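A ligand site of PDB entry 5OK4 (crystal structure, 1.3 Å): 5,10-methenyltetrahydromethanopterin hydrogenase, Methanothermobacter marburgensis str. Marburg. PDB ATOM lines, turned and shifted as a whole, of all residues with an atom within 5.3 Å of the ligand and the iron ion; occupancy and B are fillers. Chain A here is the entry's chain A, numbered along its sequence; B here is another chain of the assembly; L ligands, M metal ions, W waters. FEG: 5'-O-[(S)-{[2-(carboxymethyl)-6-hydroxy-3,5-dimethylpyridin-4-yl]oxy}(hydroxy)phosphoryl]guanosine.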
ATOM      1  N   LEU A   6     -11.193 -19.720   8.612  1.00  0.00           N
ATOM      2  CA  LEU A   6     -10.213 -19.022   7.777  1.00  0.00           C
ATOM      3  C   LEU A   6      -8.860 -19.674   8.027  1.00  0.00           C
ATOM      4  O   LEU A   6      -8.170 -19.383   9.017  1.00  0.00           O
ATOM      5  CB  LEU A   6     -10.207 -17.529   8.072  1.00  0.00           C
ATOM      6  CG  LEU A   6     -11.562 -16.828   8.008  1.00  0.00           C
ATOM      7  CD1 LEU A   6     -11.348 -15.318   8.112  1.00  0.00           C
ATOM      8  CD2 LEU A   6     -12.358 -17.152   6.824  1.00  0.00           C
ATOM      9  N   GLY A   7      -8.517 -20.599   7.137  1.00  0.00           N
ATOM     10  CA  GLY A   7      -7.303 -21.393   7.202  1.00  0.00           C
ATOM     11  C   GLY A   7      -7.625 -22.855   7.425  1.00  0.00           C
ATOM     12  O   GLY A   7      -8.128 -23.227   8.487  1.00  0.00           O
ATOM     13  N   ALA A   8      -7.344 -23.670   6.415  1.00  0.00           N
ATOM     14  CA  ALA A   8      -7.606 -25.107   6.488  1.00  0.00           C
ATOM     15  C   ALA A   8      -6.501 -25.881   7.167  1.00  0.00           C
ATOM     16  O   ALA A   8      -6.730 -27.029   7.596  1.00  0.00           O
ATOM     17  CB  ALA A   8      -7.767 -25.658   5.062  1.00  0.00           C
ATOM     18  N   GLY A   9      -5.301 -25.322   7.242  1.00  0.00           N
ATOM     19  CA  GLY A   9      -4.152 -26.004   7.800  1.00  0.00           C
ATOM     20  C   GLY A   9      -3.449 -26.917   6.809  1.00  0.00           C
ATOM     21  O   GLY A   9      -3.944 -27.234   5.734  1.00  0.00           O
ATOM     22  N   CYS A  10      -2.261 -27.344   7.211  1.00  0.00           N
ATOM     23  CA  CYS A  10      -1.509 -28.372   6.488  1.00  0.00           C
ATOM     24  C   CYS A  10      -1.041 -29.416   7.491  1.00  0.00           C
ATOM     25  O   CYS A  10      -0.626 -29.076   8.595  1.00  0.00           O
ATOM     26  CB  CYS A  10      -0.294 -27.793   5.778  1.00  0.00           C
ATOM     27  SG  CYS A  10       0.634 -29.025   4.836  1.00  0.00           S
ATOM     28  N   THR A  13       3.544 -30.456   9.294  1.00  0.00           N
ATOM     29  CA  THR A  13       4.294 -30.337  10.551  1.00  0.00           C
ATOM     30  C   THR A  13       3.769 -31.311  11.597  1.00  0.00           C
ATOM     31  O   THR A  13       4.505 -31.698  12.504  1.00  0.00           O
ATOM     32  CB  THR A  13       4.271 -28.933  11.119  1.00  0.00           C
ATOM     33  OG1 THR A  13       2.932 -28.554  11.456  1.00  0.00           O
ATOM     34  CG2 THR A  13       4.911 -27.948  10.178  1.00  0.00           C
ATOM     35  N   HIS A  14       2.496 -31.702  11.486  1.00  0.00           N
ATOM     36  CA  HIS A  14       1.987 -32.723  12.415  1.00  0.00           C
ATOM     37  C   HIS A  14       2.694 -34.039  12.157  1.00  0.00           C
ATOM     38  O   HIS A  14       3.229 -34.674  13.079  1.00  0.00           O
ATOM     39  CB  HIS A  14       0.466 -32.871  12.277  1.00  0.00           C
ATOM     40  CG  HIS A  14      -0.296 -31.604  12.544  1.00  0.00           C
ATOM     41  ND1 HIS A  14      -1.663 -31.588  12.759  1.00  0.00           N
ATOM     42  CD2 HIS A  14       0.111 -30.315  12.637  1.00  0.00           C
ATOM     43  CE1 HIS A  14      -2.058 -30.338  12.963  1.00  0.00           C
ATOM     44  NE2 HIS A  14      -1.000 -29.550  12.904  1.00  0.00           N
ATOM     45  N   SER A  42      -6.646 -30.432  12.069  1.00  0.00           N
ATOM     46  CA  SER A  42      -6.632 -28.981  12.248  1.00  0.00           C
ATOM     47  C   SER A  42      -8.060 -28.435  12.323  1.00  0.00           C
ATOM     48  O   SER A  42      -8.910 -28.997  13.035  1.00  0.00           O
ATOM     49  CB  SER A  42      -5.779 -28.332  11.205  1.00  0.00           C
ATOM     50  OG  SER A  42      -4.468 -28.877  11.210  1.00  0.00           O
ATOM     51  N   ALA A  62     -12.299 -21.003   4.096  1.00  0.00           N
ATOM     52  CA  ALA A  62     -11.598 -20.110   3.176  1.00  0.00           C
ATOM     53  C   ALA A  62     -10.098 -20.300   3.363  1.00  0.00           C
ATOM     54  O   ALA A  62      -9.595 -20.290   4.485  1.00  0.00           O
ATOM     55  CB  ALA A  62     -11.954 -18.648   3.430  1.00  0.00           C
ATOM     56  N   ASP A  63      -9.400 -20.425   2.268  1.00  0.00           N
ATOM     57  CA  ASP A  63      -7.948 -20.519   2.316  1.00  0.00           C
ATOM     58  C   ASP A  63      -7.459 -20.276   0.901  1.00  0.00           C
ATOM     59  O   ASP A  63      -8.040 -20.828  -0.046  1.00  0.00           O
ATOM     60  CB  ASP A  63      -7.573 -21.927   2.762  1.00  0.00           C
ATOM     61  CG  ASP A  63      -6.141 -22.060   3.185  1.00  0.00           C
ATOM     62  OD1 ASP A  63      -5.246 -21.633   2.444  1.00  0.00           O
ATOM     63  OD2 ASP A  63      -5.902 -22.604   4.276  1.00  0.00           O
ATOM     64  N   PRO A  64      -6.411 -19.483   0.687  1.00  0.00           N
ATOM     65  CA  PRO A  64      -5.906 -19.308  -0.683  1.00  0.00           C
ATOM     66  C   PRO A  64      -5.491 -20.613  -1.324  1.00  0.00           C
ATOM     67  O   PRO A  64      -5.444 -20.721  -2.561  1.00  0.00           O
ATOM     68  CB  PRO A  64      -4.718 -18.356  -0.509  1.00  0.00           C
ATOM     69  CG  PRO A  64      -4.951 -17.678   0.773  1.00  0.00           C
ATOM     70  CD  PRO A  64      -5.633 -18.673   1.640  1.00  0.00           C
ATOM     71  N   VAL A  65      -5.178 -21.636  -0.520  1.00  0.00           N
ATOM     72  CA  VAL A  65      -4.595 -22.843  -1.062  1.00  0.00           C
ATOM     73  C   VAL A  65      -5.566 -23.568  -1.974  1.00  0.00           C
ATOM     74  O   VAL A  65      -5.134 -24.370  -2.802  1.00  0.00           O
ATOM     75  CB  VAL A  65      -4.104 -23.760   0.074  1.00  0.00           C
ATOM     76  CG1 VAL A  65      -5.264 -24.440   0.809  1.00  0.00           C
ATOM     77  CG2 VAL A  65      -3.140 -24.774  -0.456  1.00  0.00           C
ATOM     78  N   PRO A 110       2.106 -23.991   2.762  1.00  0.00           N
ATOM     79  CA  PRO A 110       0.905 -23.174   2.638  1.00  0.00           C
ATOM     80  C   PRO A 110       1.275 -21.715   2.615  1.00  0.00           C
ATOM     81  O   PRO A 110       2.230 -21.352   3.279  1.00  0.00           O
ATOM     82  CB  PRO A 110       0.090 -23.521   3.898  1.00  0.00           C
ATOM     83  CG  PRO A 110       0.942 -24.325   4.715  1.00  0.00           C
ATOM     84  CD  PRO A 110       2.078 -24.851   3.945  1.00  0.00           C
ATOM     85  N   PRO A 111       0.525 -20.883   1.890  1.00  0.00           N
ATOM     86  CA  PRO A 111      -0.733 -21.164   1.202  1.00  0.00           C
ATOM     87  C   PRO A 111      -0.604 -21.665  -0.228  1.00  0.00           C
ATOM     88  O   PRO A 111      -1.613 -21.720  -0.911  1.00  0.00           O
ATOM     89  CB  PRO A 111      -1.449 -19.820   1.227  1.00  0.00           C
ATOM     90  CG  PRO A 111      -0.360 -18.851   1.143  1.00  0.00           C
ATOM     91  CD  PRO A 111       0.800 -19.444   1.928  1.00  0.00           C
ATOM     92  N   ALA A 114      -0.965 -27.557   0.563  1.00  0.00           N
ATOM     93  CA  ALA A 114      -1.417 -28.041   1.870  1.00  0.00           C
ATOM     94  C   ALA A 114      -1.796 -29.493   1.706  1.00  0.00           C
ATOM     95  O   ALA A 114      -2.298 -29.897   0.651  1.00  0.00           O
ATOM     96  CB  ALA A 114      -2.593 -27.255   2.423  1.00  0.00           C
ATOM     97  N   ASP A 131     -11.733 -14.658   1.648  1.00  0.00           N
ATOM     98  CA  ASP A 131     -12.079 -14.503   3.065  1.00  0.00           C
ATOM     99  C   ASP A 131     -13.268 -13.560   3.242  1.00  0.00           C
ATOM    100  O   ASP A 131     -14.053 -13.721   4.186  1.00  0.00           O
ATOM    101  CB  ASP A 131     -10.888 -13.935   3.833  1.00  0.00           C
ATOM    102  CG  ASP A 131      -9.713 -14.886   3.909  1.00  0.00           C
ATOM    103  OD1 ASP A 131      -9.875 -16.083   3.664  1.00  0.00           O
ATOM    104  OD2 ASP A 131      -8.603 -14.418   4.245  1.00  0.00           O
ATOM    105  N   TRP A 144      -7.176 -19.202  11.664  1.00  0.00           N
ATOM    106  CA  TRP A 144      -6.136 -20.202  11.855  1.00  0.00           C
ATOM    107  C   TRP A 144      -4.912 -19.757  11.049  1.00  0.00           C
ATOM    108  O   TRP A 144      -4.520 -20.375  10.071  1.00  0.00           O
ATOM    109  CB  TRP A 144      -6.633 -21.573  11.410  1.00  0.00           C
ATOM    110  CG  TRP A 144      -5.888 -22.729  11.878  1.00  0.00           C
ATOM    111  CD1 TRP A 144      -5.124 -23.568  11.121  1.00  0.00           C
ATOM    112  CD2 TRP A 144      -5.949 -23.286  13.183  1.00  0.00           C
ATOM    113  NE1 TRP A 144      -4.695 -24.613  11.891  1.00  0.00           N
ATOM    114  CE2 TRP A 144      -5.173 -24.458  13.163  1.00  0.00           C
ATOM    115  CE3 TRP A 144      -6.581 -22.905  14.365  1.00  0.00           C
ATOM    116  CZ2 TRP A 144      -5.024 -25.261  14.295  1.00  0.00           C
ATOM    117  CZ3 TRP A 144      -6.414 -23.678  15.478  1.00  0.00           C
ATOM    118  CH2 TRP A 144      -5.634 -24.844  15.445  1.00  0.00           C
ATOM    119  N   PHE A 145      -4.329 -18.664  11.481  1.00  0.00           N
ATOM    120  CA  PHE A 145      -3.344 -17.979  10.689  1.00  0.00           C
ATOM    121  C   PHE A 145      -1.924 -18.190  11.224  1.00  0.00           C
ATOM    122  O   PHE A 145      -1.741 -18.448  12.415  1.00  0.00           O
ATOM    123  CB  PHE A 145      -3.634 -16.462  10.672  1.00  0.00           C
ATOM    124  CG  PHE A 145      -4.945 -16.076  10.018  1.00  0.00           C
ATOM    125  CD1 PHE A 145      -5.492 -16.816   8.973  1.00  0.00           C
ATOM    126  CD2 PHE A 145      -5.620 -14.957  10.450  1.00  0.00           C
ATOM    127  CE1 PHE A 145      -6.681 -16.424   8.383  1.00  0.00           C
ATOM    128  CE2 PHE A 145      -6.796 -14.562   9.857  1.00  0.00           C
ATOM    129  CZ  PHE A 145      -7.334 -15.289   8.828  1.00  0.00           C
ATOM    130  N   PRO A 146      -0.997 -18.143  10.315  1.00  0.00           N
ATOM    131  CA  PRO A 146       0.384 -17.939  10.659  1.00  0.00           C
ATOM    132  C   PRO A 146       0.611 -16.804  11.633  1.00  0.00           C
ATOM    133  O   PRO A 146      -0.250 -16.135  12.205  1.00  0.00           O
ATOM    134  CB  PRO A 146       1.007 -17.578   9.301  1.00  0.00           C
ATOM    135  CG  PRO A 146       0.160 -18.271   8.312  1.00  0.00           C
ATOM    136  CD  PRO A 146      -1.196 -18.131   8.861  1.00  0.00           C
ATOM    137  N   ILE A 154      -3.783  -9.686   6.775  1.00  0.00           N
ATOM    138  CA  ILE A 154      -4.808 -10.637   6.348  1.00  0.00           C
ATOM    139  C   ILE A 154      -6.179 -10.159   6.782  1.00  0.00           C
ATOM    140  O   ILE A 154      -7.131 -10.120   6.007  1.00  0.00           O
ATOM    141  CB  ILE A 154      -4.478 -12.044   6.904  1.00  0.00           C
ATOM    142  CG1 ILE A 154      -3.190 -12.612   6.296  1.00  0.00           C
ATOM    143  CG2 ILE A 154      -5.654 -12.996   6.677  1.00  0.00           C
ATOM    144  CD1 ILE A 154      -2.640 -13.840   6.996  1.00  0.00           C
ATOM    145  N   HIS A 170      -8.799 -16.554  17.472  1.00  0.00           N
ATOM    146  CA  HIS A 170      -7.432 -16.453  16.971  1.00  0.00           C
ATOM    147  C   HIS A 170      -6.627 -17.716  17.257  1.00  0.00           C
ATOM    148  O   HIS A 170      -6.826 -18.394  18.259  1.00  0.00           O
ATOM    149  CB  HIS A 170      -6.694 -15.266  17.576  1.00  0.00           C
ATOM    150  CG  HIS A 170      -6.465 -15.380  19.038  1.00  0.00           C
ATOM    151  ND1 HIS A 170      -5.385 -16.039  19.570  1.00  0.00           N
ATOM    152  CD2 HIS A 170      -7.211 -14.952  20.071  1.00  0.00           C
ATOM    153  CE1 HIS A 170      -5.474 -16.000  20.891  1.00  0.00           C
ATOM    154  NE2 HIS A 170      -6.577 -15.357  21.216  1.00  0.00           N
ATOM    155  N   ALA A 171      -5.665 -17.973  16.380  1.00  0.00           N
ATOM    156  CA  ALA A 171      -4.688 -19.034  16.562  1.00  0.00           C
ATOM    157  C   ALA A 171      -3.681 -18.673  17.664  1.00  0.00           C
ATOM    158  O   ALA A 171      -3.510 -17.520  18.052  1.00  0.00           O
ATOM    159  CB  ALA A 171      -3.962 -19.263  15.239  1.00  0.00           C
ATOM    160  N   CYS A 172      -2.972 -19.679  18.145  1.00  0.00           N
ATOM    161  CA  CYS A 172      -2.000 -19.466  19.213  1.00  0.00           C
ATOM    162  C   CYS A 172      -0.762 -18.741  18.736  1.00  0.00           C
ATOM    163  O   CYS A 172       0.119 -18.442  19.549  1.00  0.00           O
ATOM    164  CB  CYS A 172      -1.594 -20.789  19.832  1.00  0.00           C
ATOM    165  SG  CYS A 172      -0.619 -21.869  18.734  1.00  0.00           S
ATOM    166  N   THR A 173      -0.661 -18.480  17.459  1.00  0.00           N
ATOM    167  CA  THR A 173       0.429 -17.743  16.847  1.00  0.00           C
ATOM    168  C   THR A 173       0.350 -16.253  17.156  1.00  0.00           C
ATOM    169  O   THR A 173       1.255 -15.515  16.758  1.00  0.00           O
ATOM    170  CB  THR A 173       0.350 -17.953  15.352  1.00  0.00           C
ATOM    171  OG1 THR A 173      -0.952 -17.576  14.917  1.00  0.00           O
ATOM    172  CG2 THR A 173       0.649 -19.411  14.961  1.00  0.00           C
ATOM    173  N   HIS A 203      -9.073 -22.812  20.985  1.00  0.00           N
ATOM    174  CA  HIS A 203      -7.764 -23.334  20.675  1.00  0.00           C
ATOM    175  C   HIS A 203      -7.569 -24.694  21.303  1.00  0.00           C
ATOM    176  O   HIS A 203      -7.657 -24.821  22.527  1.00  0.00           O
ATOM    177  CB  HIS A 203      -6.685 -22.392  21.137  1.00  0.00           C
ATOM    178  CG  HIS A 203      -5.331 -22.899  20.775  1.00  0.00           C
ATOM    179  ND1 HIS A 203      -4.531 -23.578  21.655  1.00  0.00           N
ATOM    180  CD2 HIS A 203      -4.659 -22.875  19.599  1.00  0.00           C
ATOM    181  CE1 HIS A 203      -3.411 -23.944  21.048  1.00  0.00           C
ATOM    182  NE2 HIS A 203      -3.468 -23.541  19.795  1.00  0.00           N
ATOM    183  N   PRO A 204      -7.254 -25.703  20.518  1.00  0.00           N
ATOM    184  CA  PRO A 204      -7.057 -27.040  21.069  1.00  0.00           C
ATOM    185  C   PRO A 204      -5.669 -27.170  21.642  1.00  0.00           C
ATOM    186  O   PRO A 204      -4.700 -26.592  21.136  1.00  0.00           O
ATOM    187  CB  PRO A 204      -7.186 -27.919  19.825  1.00  0.00           C
ATOM    188  CG  PRO A 204      -6.709 -27.040  18.694  1.00  0.00           C
ATOM    189  CD  PRO A 204      -7.121 -25.669  19.050  1.00  0.00           C
ATOM    190  N   VAL A 207      -2.823 -31.278  18.795  1.00  0.00           N
ATOM    191  CA  VAL A 207      -3.516 -31.041  17.542  1.00  0.00           C
ATOM    192  C   VAL A 207      -4.908 -31.629  17.690  1.00  0.00           C
ATOM    193  O   VAL A 207      -5.091 -32.669  18.356  1.00  0.00           O
ATOM    194  CB  VAL A 207      -2.709 -31.614  16.366  1.00  0.00           C
ATOM    195  CG1 VAL A 207      -1.372 -30.870  16.253  1.00  0.00           C
ATOM    196  CG2 VAL A 207      -2.489 -33.113  16.493  1.00  0.00           C
ATOM    197  N   ASP B 189       2.191 -26.155  20.254  1.00  0.00           N
ATOM    198  CA  ASP B 189       1.321 -27.251  20.592  1.00  0.00           C
ATOM    199  C   ASP B 189       2.000 -28.597  20.490  1.00  0.00           C
ATOM    200  O   ASP B 189       1.432 -29.589  20.935  1.00  0.00           O
ATOM    201  CB  ASP B 189       0.110 -27.246  19.667  1.00  0.00           C
ATOM    202  CG  ASP B 189      -0.615 -25.916  19.706  1.00  0.00           C
ATOM    203  OD1 ASP B 189      -0.664 -25.301  20.809  1.00  0.00           O
ATOM    204  OD2 ASP B 189      -1.104 -25.453  18.641  1.00  0.00           O
HETATM  205  N1  FEG L   1      -1.686 -24.882  14.186  1.00  0.00           N
HETATM  206  C2  FEG L   1      -0.983 -25.762  13.489  1.00  0.00           C
HETATM  207  O2  FEG L   1      -0.802 -26.973  13.983  1.00  0.00           O
HETATM  208  C3  FEG L   1      -0.399 -25.408  12.222  1.00  0.00           C
HETATM  209  C3M FEG L   1       0.417 -26.408  11.483  1.00  0.00           C
HETATM  210  C4  FEG L   1      -0.681 -24.095  11.700  1.00  0.00           C
HETATM  211  C5  FEG L   1      -1.435 -23.166  12.487  1.00  0.00           C
HETATM  212  C5M FEG L   1      -1.723 -21.804  11.914  1.00  0.00           C
HETATM  213  C6  FEG L   1      -1.924 -23.633  13.776  1.00  0.00           C
HETATM  214  C7  FEG L   1      -2.751 -22.707  14.606  1.00  0.00           C
HETATM  215  C8  FEG L   1      -2.828 -22.992  16.081  1.00  0.00           C
HETATM  216  O28 FEG L   1      -2.284 -23.998  16.587  1.00  0.00           O
HETATM  217  O18 FEG L   1      -3.425 -22.130  16.776  1.00  0.00           O
HETATM  218  O3P FEG L   1      -0.192 -23.723  10.494  1.00  0.00           O
HETATM  219  P1  FEG L   1      -0.843 -24.210   9.118  1.00  0.00           P
HETATM  220  O1P FEG L   1       0.188 -23.879   8.077  1.00  0.00           O
HETATM  221  O2P FEG L   1      -1.306 -25.611   9.256  1.00  0.00           O
HETATM  222  O5S FEG L   1      -2.147 -23.291   8.924  1.00  0.00           O
HETATM  223  C5S FEG L   1      -2.091 -21.948   8.427  1.00  0.00           C
HETATM  224  C4S FEG L   1      -3.169 -21.840   7.355  1.00  0.00           C
HETATM  225  C3S FEG L   1      -2.773 -22.520   6.038  1.00  0.00           C
HETATM  226  O3S FEG L   1      -3.737 -23.468   5.590  1.00  0.00           O
HETATM  227  C2S FEG L   1      -2.636 -21.321   5.094  1.00  0.00           C
HETATM  228  O2S FEG L   1      -2.761 -21.588   3.712  1.00  0.00           O
HETATM  229  C1S FEG L   1      -3.680 -20.380   5.664  1.00  0.00           C
HETATM  230  O4S FEG L   1      -3.398 -20.466   7.049  1.00  0.00           O
HETATM  231  N9A FEG L   1      -3.571 -18.991   5.220  1.00  0.00           N
HETATM  232  C8A FEG L   1      -2.436 -18.283   4.949  1.00  0.00           C
HETATM  233  N7A FEG L   1      -2.787 -17.046   4.549  1.00  0.00           N
HETATM  234  C5A FEG L   1      -4.132 -16.971   4.572  1.00  0.00           C
HETATM  235  C4A FEG L   1      -4.629 -18.246   5.038  1.00  0.00           C
HETATM  236  C6A FEG L   1      -5.121 -15.962   4.278  1.00  0.00           C
HETATM  237  O6A FEG L   1      -4.824 -14.819   3.851  1.00  0.00           O
HETATM  238  N1A FEG L   1      -6.400 -16.333   4.485  1.00  0.00           N
HETATM  239  C2A FEG L   1      -6.779 -17.551   4.900  1.00  0.00           C
HETATM  240  N3A FEG L   1      -5.922 -18.543   5.179  1.00  0.00           N
HETATM  241  N2A FEG L   1      -8.093 -17.787   5.040  1.00  0.00           N
HETATM  242 FE    FE M   1      -1.944 -23.700  18.520  1.00  0.00          FE
HETATM  243  O   HOH W   1       0.960 -27.511  15.876  1.00  0.00           O
HETATM  244  O   HOH W   2      -6.758 -14.693   1.289  1.00  0.00           O
HETATM  245  O   HOH W   3       1.883 -21.115  11.083  1.00  0.00           O
HETATM  246  O   HOH W   4       2.373 -25.555   8.152  1.00  0.00           O
HETATM  247  O   HOH W   5      -3.408 -28.155  14.761  1.00  0.00           O
HETATM  248  O   HOH W   6       1.870 -28.111   9.022  1.00  0.00           O
HETATM  249  O   HOH W   7      -2.742 -13.918   2.553  1.00  0.00           O
HETATM  250  O   HOH W   8       1.634 -21.674   7.671  1.00  0.00           O
HETATM  251  O   HOH W   9      -2.886 -26.742  11.192  1.00  0.00           O
HETATM  252  O   HOH W  10      -5.467 -12.201   2.510  1.00  0.00           O
HETATM  253  O   HOH W  11      -0.423 -15.668   3.991  1.00  0.00           O
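An oxygen (O18) of the ligand sits at hydrogen-bond distance from the backbone NH (N) of Cys 172, at 2.8 Å. O3S of the ligand lies within hydrogen-bond range of OD2 of Asp 63 (2.7 Å). A ring nitrogen (NE2) of His 14 sits at hydrogen-bond distance from an oxygen (O2) of the ligand, 2.8 Å away. OD1 of Asp 131 sits at hydrogen-bond distance from N2A of the ligand, 2.8 Å away. N of Cys 10 is in hydrogen-bond range of O2P of the ligand. An oxygen (O3S) of the ligand sits at hydrogen-bond distance from the backbone NH (N) of Gly 9. O of Ala 62 sits at hydrogen-bond distance from N2A of the ligand (3.0 Å).
Of the 28 residues printed, 3 come within 4 Å of the iron ion.
The backbone carbonyl oxygen of Trp 144 sits close to an oxygen (O4S) of the ligand, at 3.2 Å. Leu 6 touches the ligand. Gly 7 touches the ligand (N to N2A, 3.5 Å). N of Ala 8 touches O3S of the ligand (3.7 Å). OG1 of Thr 13 touches C3M of the ligand (3.3 Å). Pro 64 touches the ligand (CD to N3A, 3.6 Å). Pro 110 touches the ligand. CA of Pro 111 touches O2S of the ligand, 3.3 Å away. Phe 145 touches the ligand (O to C5M, 3.4 Å). Pro 146 touches the ligand (CD to O4S, 3.7 Å). Ile 154 touches the ligand (CG2 to O6A, 3.5 Å). CB of Ala 171 touches O18 of the ligand, at 3.3 Å. Hydrophobic or aromatic side chains that line the ligand: Leu 6, His 14, Pro 64, Pro 110, Pro 111, Trp 144, Phe 145, Pro 146, Ile 154, Ala 171 and His 203. The nearest printed residue that does not touch the ligand is Val 65 (4.4 Å).
Water W9 lies within hydrogen-bond range of OG of Ser 42, O2P of the ligand and NE1 of Trp 144. Water W5 bridges an oxygen (O2) of the ligand (3.0 Å) and a ring nitrogen (NE2) of His 14 (3.3 Å). Water W2 bridges O6A of the ligand and OD2 of Asp 131. Water W6 bridges OG1 of Thr 13 (2.7 Å) and O of Cys 10 (2.7 Å).
The backbone NH of Ala 8 is in hydrogen-bond range of the side-chain carboxylate of Asp 63, at 2.8 Å. The backbone NH (N) of Val 65 lies within hydrogen-bond range of the side-chain carboxylate (OD1) of Asp 63 (3.0 Å). The backbone NH (N) of Gly 7 lies within hydrogen-bond range of the backbone carbonyl oxygen (O) of Ala 62, 2.9 Å away. The backbone NH (N) of Trp 144 is in hydrogen-bond range of the backbone carbonyl oxygen (O) of Leu 6 (2.8 Å). OG1 of Thr 173 is in hydrogen-bond range of O of Phe 145, at 2.8 Å. O of Pro 146 sits at hydrogen-bond distance from OG1 of Thr 173, at 3.2 Å.
OD2 of Asp 189 of chain B is bound to the iron ion. An oxygen (O28) of the ligand is bound to the iron ion (2.0 Å). NE2 of His 203 is bound to the iron ion (2.0 Å). The iron ion is bound by SG of Cys 172 (2.3 Å). The iron ion has four donor atoms within binding distance. Slightly farther from the iron ion lies O18 of the ligand (2.8 Å).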
